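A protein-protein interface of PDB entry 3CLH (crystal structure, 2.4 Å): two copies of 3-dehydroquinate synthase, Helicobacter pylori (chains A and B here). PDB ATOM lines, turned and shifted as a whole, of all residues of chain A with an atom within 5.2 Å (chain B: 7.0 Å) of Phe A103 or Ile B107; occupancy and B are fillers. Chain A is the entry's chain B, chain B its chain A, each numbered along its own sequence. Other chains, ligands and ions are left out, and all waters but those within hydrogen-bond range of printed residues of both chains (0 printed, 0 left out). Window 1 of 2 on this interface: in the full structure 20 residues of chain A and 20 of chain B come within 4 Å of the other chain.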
ATOM      1  N   LEU A  71      18.494   0.700  10.505  1.00  0.00           N
ATOM      2  CA  LEU A  71      19.239   1.830   9.952  1.00  0.00           C
ATOM      3  C   LEU A  71      18.604   3.160  10.359  1.00  0.00           C
ATOM      4  O   LEU A  71      19.309   4.119  10.674  1.00  0.00           O
ATOM      5  CB  LEU A  71      19.317   1.723   8.425  1.00  0.00           C
ATOM      6  CG  LEU A  71      20.139   2.760   7.654  1.00  0.00           C
ATOM      7  CD1 LEU A  71      21.625   2.433   7.704  1.00  0.00           C
ATOM      8  CD2 LEU A  71      19.657   2.845   6.217  1.00  0.00           C
ATOM      9  N   SER A  98      28.952  -3.178  11.393  1.00  0.00           N
ATOM     10  CA  SER A  98      29.893  -2.336  10.644  1.00  0.00           C
ATOM     11  C   SER A  98      29.354  -1.861   9.291  1.00  0.00           C
ATOM     12  O   SER A  98      29.674  -0.756   8.846  1.00  0.00           O
ATOM     13  CB  SER A  98      31.228  -3.062  10.454  1.00  0.00           C
ATOM     14  OG  SER A  98      31.062  -4.252   9.704  1.00  0.00           O
ATOM     15  N   ASP A  99      28.544  -2.698   8.646  1.00  0.00           N
ATOM     16  CA  ASP A  99      27.913  -2.348   7.373  1.00  0.00           C
ATOM     17  C   ASP A  99      26.766  -1.355   7.552  1.00  0.00           C
ATOM     18  O   ASP A  99      26.578  -0.465   6.722  1.00  0.00           O
ATOM     19  CB  ASP A  99      27.416  -3.601   6.644  1.00  0.00           C
ATOM     20  CG  ASP A  99      28.542  -4.401   6.005  1.00  0.00           C
ATOM     21  OD1 ASP A  99      29.706  -4.279   6.446  1.00  0.00           O
ATOM     22  OD2 ASP A  99      28.257  -5.164   5.057  1.00  0.00           O
ATOM     23  N   MET A 100      26.004  -1.514   8.633  1.00  0.00           N
ATOM     24  CA  MET A 100      24.879  -0.626   8.931  1.00  0.00           C
ATOM     25  C   MET A 100      25.337   0.751   9.406  1.00  0.00           C
ATOM     26  O   MET A 100      24.803   1.770   8.968  1.00  0.00           O
ATOM     27  CB  MET A 100      23.938  -1.252   9.965  1.00  0.00           C
ATOM     28  CG  MET A 100      23.028  -2.341   9.411  1.00  0.00           C
ATOM     29  SD  MET A 100      21.622  -2.710  10.483  1.00  0.00           S
ATOM     30  CE  MET A 100      22.429  -3.478  11.888  1.00  0.00           C
ATOM     31  N   VAL A 101      26.327   0.766  10.300  1.00  0.00           N
ATOM     32  CA  VAL A 101      26.888   2.007  10.845  1.00  0.00           C
ATOM     33  C   VAL A 101      27.598   2.814   9.756  1.00  0.00           C
ATOM     34  O   VAL A 101      27.425   4.031   9.666  1.00  0.00           O
ATOM     35  CB  VAL A 101      27.853   1.726  12.030  1.00  0.00           C
ATOM     36  CG1 VAL A 101      28.528   3.005  12.511  1.00  0.00           C
ATOM     37  CG2 VAL A 101      27.110   1.066  13.177  1.00  0.00           C
ATOM     38  N   GLY A 102      28.384   2.123   8.933  1.00  0.00           N
ATOM     39  CA  GLY A 102      29.107   2.749   7.829  1.00  0.00           C
ATOM     40  C   GLY A 102      28.198   3.358   6.776  1.00  0.00           C
ATOM     41  O   GLY A 102      28.523   4.393   6.193  1.00  0.00           O
ATOM     42  N   PHE A 103      27.059   2.710   6.534  1.00  0.00           N
ATOM     43  CA  PHE A 103      26.057   3.225   5.603  1.00  0.00           C
ATOM     44  C   PHE A 103      25.221   4.340   6.234  1.00  0.00           C
ATOM     45  O   PHE A 103      24.780   5.257   5.538  1.00  0.00           O
ATOM     46  CB  PHE A 103      25.160   2.094   5.079  1.00  0.00           C
ATOM     47  CG  PHE A 103      24.129   2.543   4.073  1.00  0.00           C
ATOM     48  CD1 PHE A 103      24.501   3.265   2.942  1.00  0.00           C
ATOM     49  CD2 PHE A 103      22.785   2.231   4.252  1.00  0.00           C
ATOM     50  CE1 PHE A 103      23.550   3.682   2.014  1.00  0.00           C
ATOM     51  CE2 PHE A 103      21.827   2.639   3.327  1.00  0.00           C
ATOM     52  CZ  PHE A 103      22.210   3.365   2.206  1.00  0.00           C
ATOM     53  N   ALA A 104      25.015   4.257   7.547  1.00  0.00           N
ATOM     54  CA  ALA A 104      24.292   5.293   8.288  1.00  0.00           C
ATOM     55  C   ALA A 104      25.108   6.579   8.392  1.00  0.00           C
ATOM     56  O   ALA A 104      24.562   7.676   8.270  1.00  0.00           O
ATOM     57  CB  ALA A 104      23.905   4.794   9.671  1.00  0.00           C
ATOM     58  N   SER A 105      26.414   6.433   8.612  1.00  0.00           N
ATOM     59  CA  SER A 105      27.327   7.571   8.724  1.00  0.00           C
ATOM     60  C   SER A 105      27.583   8.250   7.380  1.00  0.00           C
ATOM     61  O   SER A 105      27.862   9.449   7.331  1.00  0.00           O
ATOM     62  CB  SER A 105      28.653   7.137   9.353  1.00  0.00           C
ATOM     63  OG  SER A 105      29.270   6.113   8.592  1.00  0.00           O
ATOM     64  N   SER A 106      27.485   7.480   6.298  1.00  0.00           N
ATOM     65  CA  SER A 106      27.699   7.996   4.946  1.00  0.00           C
ATOM     66  C   SER A 106      26.562   8.904   4.480  1.00  0.00           C
ATOM     67  O   SER A 106      26.773   9.802   3.662  1.00  0.00           O
ATOM     68  CB  SER A 106      27.881   6.846   3.953  1.00  0.00           C
ATOM     69  OG  SER A 106      26.705   6.064   3.849  1.00  0.00           O
ATOM     70  N   ILE A 107      25.361   8.660   5.000  1.00  0.00           N
ATOM     71  CA  ILE A 107      24.169   9.404   4.585  1.00  0.00           C
ATOM     72  C   ILE A 107      23.730  10.473   5.594  1.00  0.00           C
ATOM     73  O   ILE A 107      22.981  11.389   5.246  1.00  0.00           O
ATOM     74  CB  ILE A 107      22.979   8.461   4.234  1.00  0.00           C
ATOM     75  CG1 ILE A 107      22.511   7.672   5.465  1.00  0.00           C
ATOM     76  CG2 ILE A 107      23.355   7.532   3.076  1.00  0.00           C
ATOM     77  CD1 ILE A 107      21.154   7.005   5.305  1.00  0.00           C
ATOM     78  N   THR A 133      29.797  -0.858   2.482  1.00  0.00           N
ATOM     79  CA  THR A 133      28.702  -0.851   3.452  1.00  0.00           C
ATOM     80  C   THR A 133      27.350  -1.062   2.773  1.00  0.00           C
ATOM     81  O   THR A 133      27.215  -0.842   1.567  1.00  0.00           O
ATOM     82  CB  THR A 133      28.674   0.468   4.261  1.00  0.00           C
ATOM     83  OG1 THR A 133      28.469   1.576   3.375  1.00  0.00           O
ATOM     84  CG2 THR A 133      29.979   0.664   5.024  1.00  0.00           C
ATOM     85  N   GLY A 134      26.355  -1.493   3.548  1.00  0.00           N
ATOM     86  CA  GLY A 134      25.008  -1.702   3.021  1.00  0.00           C
ATOM     87  C   GLY A 134      24.028  -2.386   3.955  1.00  0.00           C
ATOM     88  O   GLY A 134      24.389  -2.815   5.053  1.00  0.00           O
ATOM     89  N   ILE A 135      22.777  -2.473   3.504  1.00  0.00           N
ATOM     90  CA  ILE A 135      21.702  -3.152   4.234  1.00  0.00           C
ATOM     91  C   ILE A 135      20.942  -4.108   3.309  1.00  0.00           C
ATOM     92  O   ILE A 135      21.027  -3.995   2.084  1.00  0.00           O
ATOM     93  CB  ILE A 135      20.704  -2.151   4.885  1.00  0.00           C
ATOM     94  CG1 ILE A 135      20.203  -1.125   3.857  1.00  0.00           C
ATOM     95  CG2 ILE A 135      21.341  -1.467   6.096  1.00  0.00           C
ATOM     96  CD1 ILE A 135      18.901  -0.438   4.238  1.00  0.00           C
ATOM     97  N   LEU A 143      22.076  -4.783  -1.471  1.00  0.00           N
ATOM     98  CA  LEU A 143      21.788  -4.129  -2.747  1.00  0.00           C
ATOM     99  C   LEU A 143      21.614  -2.616  -2.600  1.00  0.00           C
ATOM    100  O   LEU A 143      21.661  -1.879  -3.588  1.00  0.00           O
ATOM    101  CB  LEU A 143      20.563  -4.760  -3.424  1.00  0.00           C
ATOM    102  CG  LEU A 143      20.625  -6.252  -3.788  1.00  0.00           C
ATOM    103  CD1 LEU A 143      19.314  -6.706  -4.408  1.00  0.00           C
ATOM    104  CD2 LEU A 143      21.793  -6.573  -4.720  1.00  0.00           C
ATOM    105  N   ILE A 144      21.411  -2.163  -1.365  1.00  0.00           N
ATOM    106  CA  ILE A 144      21.362  -0.736  -1.050  1.00  0.00           C
ATOM    107  C   ILE A 144      22.483  -0.393  -0.068  1.00  0.00           C
ATOM    108  O   ILE A 144      22.456  -0.810   1.093  1.00  0.00           O
ATOM    109  CB  ILE A 144      19.975  -0.302  -0.486  1.00  0.00           C
ATOM    110  CG1 ILE A 144      18.849  -0.583  -1.498  1.00  0.00           C
ATOM    111  CG2 ILE A 144      19.984   1.173  -0.055  1.00  0.00           C
ATOM    112  CD1 ILE A 144      18.971   0.146  -2.837  1.00  0.00           C
ATOM    113  N   GLY A 145      23.470   0.360  -0.550  1.00  0.00           N
ATOM    114  CA  GLY A 145      24.626   0.738   0.259  1.00  0.00           C
ATOM    115  C   GLY A 145      25.457   1.856  -0.340  1.00  0.00           C
ATOM    116  O   GLY A 145      24.999   2.572  -1.231  1.00  0.00           O
ATOM    117  N   SER A 146      26.685   2.001   0.157  1.00  0.00           N
ATOM    118  CA  SER A 146      27.612   3.032  -0.313  1.00  0.00           C
ATOM    119  C   SER A 146      29.064   2.679   0.009  1.00  0.00           C
ATOM    120  O   SER A 146      29.332   1.867   0.897  1.00  0.00           O
ATOM    121  CB  SER A 146      27.261   4.394   0.301  1.00  0.00           C
ATOM    122  OG  SER A 146      27.350   4.355   1.716  1.00  0.00           O
ATOM    123  N   LEU B  71      11.414   8.138  -2.031  1.00  0.00           N
ATOM    124  CA  LEU B  71      12.744   7.581  -2.275  1.00  0.00           C
ATOM    125  C   LEU B  71      12.695   6.057  -2.396  1.00  0.00           C
ATOM    126  O   LEU B  71      13.384   5.474  -3.235  1.00  0.00           O
ATOM    127  CB  LEU B  71      13.709   7.993  -1.156  1.00  0.00           C
ATOM    128  CG  LEU B  71      15.186   7.604  -1.276  1.00  0.00           C
ATOM    129  CD1 LEU B  71      15.928   8.536  -2.228  1.00  0.00           C
ATOM    130  CD2 LEU B  71      15.841   7.608   0.093  1.00  0.00           C
ATOM    131  N   LEU B  75      13.594   3.581  -5.722  1.00  0.00           N
ATOM    132  CA  LEU B  75      14.444   2.400  -5.580  1.00  0.00           C
ATOM    133  C   LEU B  75      13.719   1.123  -6.003  1.00  0.00           C
ATOM    134  O   LEU B  75      14.292   0.287  -6.703  1.00  0.00           O
ATOM    135  CB  LEU B  75      14.957   2.264  -4.141  1.00  0.00           C
ATOM    136  CG  LEU B  75      15.894   3.340  -3.580  1.00  0.00           C
ATOM    137  CD1 LEU B  75      15.965   3.232  -2.064  1.00  0.00           C
ATOM    138  CD2 LEU B  75      17.287   3.265  -4.197  1.00  0.00           C
ATOM    139  N   VAL B 101      16.444  11.619  -6.906  1.00  0.00           N
ATOM    140  CA  VAL B 101      17.021  10.703  -7.895  1.00  0.00           C
ATOM    141  C   VAL B 101      18.529  10.552  -7.685  1.00  0.00           C
ATOM    142  O   VAL B 101      19.060   9.440  -7.740  1.00  0.00           O
ATOM    143  CB  VAL B 101      16.726  11.165  -9.349  1.00  0.00           C
ATOM    144  CG1 VAL B 101      17.365  10.225 -10.369  1.00  0.00           C
ATOM    145  CG2 VAL B 101      15.230  11.250  -9.590  1.00  0.00           C
ATOM    146  N   GLY B 102      19.202  11.673  -7.432  1.00  0.00           N
ATOM    147  CA  GLY B 102      20.641  11.685  -7.182  1.00  0.00           C
ATOM    148  C   GLY B 102      21.044  10.910  -5.940  1.00  0.00           C
ATOM    149  O   GLY B 102      22.094  10.264  -5.919  1.00  0.00           O
ATOM    150  N   PHE B 103      20.209  10.978  -4.904  1.00  0.00           N
ATOM    151  CA  PHE B 103      20.443  10.230  -3.669  1.00  0.00           C
ATOM    152  C   PHE B 103      20.058   8.758  -3.819  1.00  0.00           C
ATOM    153  O   PHE B 103      20.688   7.886  -3.218  1.00  0.00           O
ATOM    154  CB  PHE B 103      19.706  10.873  -2.486  1.00  0.00           C
ATOM    155  CG  PHE B 103      19.933  10.175  -1.168  1.00  0.00           C
ATOM    156  CD1 PHE B 103      21.224   9.948  -0.695  1.00  0.00           C
ATOM    157  CD2 PHE B 103      18.856   9.758  -0.394  1.00  0.00           C
ATOM    158  CE1 PHE B 103      21.436   9.303   0.520  1.00  0.00           C
ATOM    159  CE2 PHE B 103      19.059   9.116   0.826  1.00  0.00           C
ATOM    160  CZ  PHE B 103      20.351   8.889   1.283  1.00  0.00           C
ATOM    161  N   ALA B 104      19.027   8.492  -4.619  1.00  0.00           N
ATOM    162  CA  ALA B 104      18.590   7.122  -4.896  1.00  0.00           C
ATOM    163  C   ALA B 104      19.607   6.371  -5.754  1.00  0.00           C
ATOM    164  O   ALA B 104      19.834   5.179  -5.549  1.00  0.00           O
ATOM    165  CB  ALA B 104      17.224   7.118  -5.564  1.00  0.00           C
ATOM    166  N   SER B 105      20.212   7.078  -6.707  1.00  0.00           N
ATOM    167  CA  SER B 105      21.227   6.500  -7.589  1.00  0.00           C
ATOM    168  C   SER B 105      22.552   6.256  -6.867  1.00  0.00           C
ATOM    169  O   SER B 105      23.298   5.344  -7.225  1.00  0.00           O
ATOM    170  CB  SER B 105      21.451   7.393  -8.813  1.00  0.00           C
ATOM    171  OG  SER B 105      21.869   8.693  -8.431  1.00  0.00           O
ATOM    172  N   SER B 106      22.834   7.075  -5.855  1.00  0.00           N
ATOM    173  CA  SER B 106      24.064   6.955  -5.073  1.00  0.00           C
ATOM    174  C   SER B 106      24.053   5.738  -4.148  1.00  0.00           C
ATOM    175  O   SER B 106      25.109   5.198  -3.812  1.00  0.00           O
ATOM    176  CB  SER B 106      24.310   8.226  -4.257  1.00  0.00           C
ATOM    177  OG  SER B 106      23.299   8.419  -3.283  1.00  0.00           O
ATOM    178  N   ILE B 107      22.857   5.315  -3.741  1.00  0.00           N
ATOM    179  CA  ILE B 107      22.707   4.189  -2.814  1.00  0.00           C
ATOM    180  C   ILE B 107      22.337   2.870  -3.501  1.00  0.00           C
ATOM    181  O   ILE B 107      22.602   1.792  -2.963  1.00  0.00           O
ATOM    182  CB  ILE B 107      21.720   4.505  -1.649  1.00  0.00           C
ATOM    183  CG1 ILE B 107      20.307   4.794  -2.179  1.00  0.00           C
ATOM    184  CG2 ILE B 107      22.252   5.661  -0.797  1.00  0.00           C
ATOM    185  CD1 ILE B 107      19.228   4.816  -1.109  1.00  0.00           C
ATOM    186  N   TYR B 108      21.730   2.963  -4.684  1.00  0.00           N
ATOM    187  CA  TYR B 108      21.322   1.786  -5.452  1.00  0.00           C
ATOM    188  C   TYR B 108      22.540   1.071  -6.031  1.00  0.00           C
ATOM    189  O   TYR B 108      23.283   1.646  -6.832  1.00  0.00           O
ATOM    190  CB  TYR B 108      20.345   2.184  -6.563  1.00  0.00           C
ATOM    191  CG  TYR B 108      19.681   1.018  -7.259  1.00  0.00           C
ATOM    192  CD1 TYR B 108      18.605   0.352  -6.672  1.00  0.00           C
ATOM    193  CD2 TYR B 108      20.121   0.586  -8.508  1.00  0.00           C
ATOM    194  CE1 TYR B 108      17.990  -0.720  -7.309  1.00  0.00           C
ATOM    195  CE2 TYR B 108      19.511  -0.482  -9.153  1.00  0.00           C
ATOM    196  CZ  TYR B 108      18.447  -1.132  -8.548  1.00  0.00           C
ATOM    197  OH  TYR B 108      17.840  -2.190  -9.183  1.00  0.00           O
ATOM    198  N   PHE B 109      22.732  -0.182  -5.612  1.00  0.00           N
ATOM    199  CA  PHE B 109      23.919  -0.984  -5.952  1.00  0.00           C
ATOM    200  C   PHE B 109      25.229  -0.260  -5.618  1.00  0.00           C
ATOM    201  O   PHE B 109      26.219  -0.368  -6.349  1.00  0.00           O
ATOM    202  CB  PHE B 109      23.881  -1.444  -7.418  1.00  0.00           C
ATOM    203  CG  PHE B 109      23.094  -2.708  -7.640  1.00  0.00           C
ATOM    204  CD1 PHE B 109      21.702  -2.689  -7.642  1.00  0.00           C
ATOM    205  CD2 PHE B 109      23.746  -3.918  -7.852  1.00  0.00           C
ATOM    206  CE1 PHE B 109      20.971  -3.855  -7.849  1.00  0.00           C
ATOM    207  CE2 PHE B 109      23.023  -5.092  -8.061  1.00  0.00           C
ATOM    208  CZ  PHE B 109      21.634  -5.060  -8.060  1.00  0.00           C
ATOM    209  N   ARG B 110      25.209   0.472  -4.502  1.00  0.00           N
ATOM    210  CA  ARG B 110      26.355   1.238  -3.991  1.00  0.00           C
ATOM    211  C   ARG B 110      26.869   2.335  -4.936  1.00  0.00           C
ATOM    212  O   ARG B 110      28.032   2.741  -4.854  1.00  0.00           O
ATOM    213  CB  ARG B 110      27.495   0.305  -3.552  1.00  0.00           C
ATOM    214  CG  ARG B 110      27.158  -0.573  -2.358  1.00  0.00           C
ATOM    215  CD  ARG B 110      28.375  -1.341  -1.878  1.00  0.00           C
ATOM    216  NE  ARG B 110      28.053  -2.228  -0.763  1.00  0.00           N
ATOM    217  CZ  ARG B 110      27.689  -3.502  -0.889  1.00  0.00           C
ATOM    218  NH1 ARG B 110      27.591  -4.062  -2.088  1.00  0.00           N
ATOM    219  NH2 ARG B 110      27.422  -4.219   0.194  1.00  0.00           N
ATOM    220  N   GLY B 111      25.996   2.815  -5.820  1.00  0.00           N
ATOM    221  CA  GLY B 111      26.334   3.916  -6.719  1.00  0.00           C
ATOM    222  C   GLY B 111      26.213   3.589  -8.195  1.00  0.00           C
ATOM    223  O   GLY B 111      26.975   2.779  -8.726  1.00  0.00           O
ATOM    224  N   ILE B 112      25.244   4.225  -8.851  1.00  0.00           N
ATOM    225  CA  ILE B 112      25.061   4.110 -10.302  1.00  0.00           C
ATOM    226  C   ILE B 112      25.028   5.495 -10.955  1.00  0.00           C
ATOM    227  O   ILE B 112      24.819   6.503 -10.277  1.00  0.00           O
ATOM    228  CB  ILE B 112      23.784   3.302 -10.683  1.00  0.00           C
ATOM    229  CG1 ILE B 112      22.514   3.980 -10.150  1.00  0.00           C
ATOM    230  CG2 ILE B 112      23.892   1.858 -10.193  1.00  0.00           C
ATOM    231  CD1 ILE B 112      21.228   3.515 -10.814  1.00  0.00           C
ATOM    232  N   GLY B 145      21.397  12.666   3.068  1.00  0.00           N
ATOM    233  CA  GLY B 145      21.775  12.718   1.658  1.00  0.00           C
ATOM    234  C   GLY B 145      23.190  12.245   1.383  1.00  0.00           C
ATOM    235  O   GLY B 145      23.800  11.573   2.217  1.00  0.00           O
ATOM    236  N   SER B 146      23.706  12.597   0.207  1.00  0.00           N
ATOM    237  CA  SER B 146      25.055  12.208  -0.210  1.00  0.00           C
ATOM    238  C   SER B 146      25.615  13.138  -1.287  1.00  0.00           C
ATOM    239  O   SER B 146      24.873  13.898  -1.912  1.00  0.00           O
ATOM    240  CB  SER B 146      25.066  10.760  -0.717  1.00  0.00           C
ATOM    241  OG  SER B 146      24.226  10.608  -1.849  1.00  0.00           O
ATOM    242  N   HIS B 148      26.869  13.035  -4.762  1.00  0.00           N
ATOM    243  CA  HIS B 148      26.861  12.191  -5.953  1.00  0.00           C
ATOM    244  C   HIS B 148      26.865  13.036  -7.226  1.00  0.00           C
ATOM    245  O   HIS B 148      25.897  13.744  -7.519  1.00  0.00           O
ATOM    246  CB  HIS B 148      25.655  11.246  -5.926  1.00  0.00           C
ATOM    247  CG  HIS B 148      25.721  10.145  -6.939  1.00  0.00           C
ATOM    248  ND1 HIS B 148      26.695   9.169  -6.919  1.00  0.00           N
ATOM    249  CD2 HIS B 148      24.920   9.852  -7.990  1.00  0.00           C
ATOM    250  CE1 HIS B 148      26.499   8.332  -7.921  1.00  0.00           C
ATOM    251  NE2 HIS B 148      25.427   8.723  -8.586  1.00  0.00           N
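No residue of chain B comes within 4 Å of Gly A102. Phe A103 touches just one residue of chain B: Ile B107 (3.7 Å). Of the printed residues of chain B, Ser A106 touches Gly B145 (3.8 Å). Of chain A, only Phe A103 (3.7 Å), Leu A143 (3.8 Å), Ile A144 (3.4 Å) and Gly A145 (2.9 Å) come within 4 Å of Ile B107. Printed residues of chain A within 4 Å of Tyr B108: Leu A143 (3.9 Å) and Ile A144 (3.9 Å). The nearest residue of chain B that does not touch Phe A103 is Phe B103 (5.9 Å). The nearest residue of chain A that does not touch Ile B107 is Ile A107 (4.4 Å). The nearest printed residue of chain B that does not touch Gly A145 is Gly B111 (4.7 Å).
Of the 17 printed residues of chain B, 8 touch a printed residue of chain A. Hydrophobic or aromatic side chains of chain B within 4 Å of the printed part of chain A: Leu B75, Phe B103, Ile B107, Tyr B108 and Phe B109. Printed residues of chain A that touch a printed residue of chain B: Phe A103, Ser A106, Ile A107, Thr A133, Leu A143, Ile A144, Gly A145 and Ser A146.
Phe A103 touches Ile B107, and with the chains exchanged Ile A107 touches Phe B103. Ser A106 touches Gly B145, and with the chains exchanged Gly A145 touches Ser B106. Ile A107 touches Gly B145, and with the chains exchanged Gly A145 touches Ile B107. Positions printed for both chains: 71, 101, 102, 103, 104, 105, 106, 107, 145 and 146. Of the 15 pairs that touch across the chains among the printed residues, 6 have their exchanged pair printed and touching as well.
The backbone carbonyl oxygen (O) of Gly A102 sits close to the side-chain hydroxyl (OG) of Ser A106, at 3.4 Å. The side-chain hydroxyl (OG) of Ser A146 lies within hydrogen-bond range of the side-chain hydroxyl (OG) of Ser A106. The backbone carbonyl oxygen (O) of Phe B103 lies within hydrogen-bond range of the side-chain hydroxyl (OG) of Ser B106 (2.7 Å). The backbone carbonyl oxygen of Ser B106 is in hydrogen-bond range of the backbone NH of Gly B111 (3.2 Å). The side-chain hydroxyl (OG) of Ser B106 is in hydrogen-bond range of the side-chain hydroxyl (OG) of Ser B146, 2.8 Å away. The side-chain hydroxyl (OG) of Ser B106 lies within hydrogen-bond range of the backbone carbonyl oxygen (O) of Gly B102, at 3.4 Å.
Among the printed residues, merely in contact across the chains: Phe A103 with Ile B107 (3.7 Å), Ser A106 with Gly B145 (3.8 Å), Ile A107 with Phe B103 (3.7 Å), Leu A143 with Ile B107 (3.8 Å), Leu A143 with Tyr B108 (3.9 Å), Ile A144 with Leu B75 (3.8 Å), Ile A144 with Ile B107 (3.4 Å), Ile A144 with Tyr B108 (3.9 Å), Gly A145 with Ser B106 (3.7 Å), Gly A145 with Arg B110 (3.4 Å) and Ser A146 with Arg B110 (3.6 Å).
O of Ile B107 is in hydrogen-bond range of N of Gly A145 (2.9 Å). O of Ile A107 sits at hydrogen-bond distance from N of Gly B145, 3.0 Å away. The backbone NH (N) of Phe B109 is in hydrogen-bond range of the backbone carbonyl oxygen (O) of Leu A143 (2.9 Å). The backbone carbonyl oxygen of Thr A133 is in hydrogen-bond range of the guanidinium group of Arg B110 (2.8 Å).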
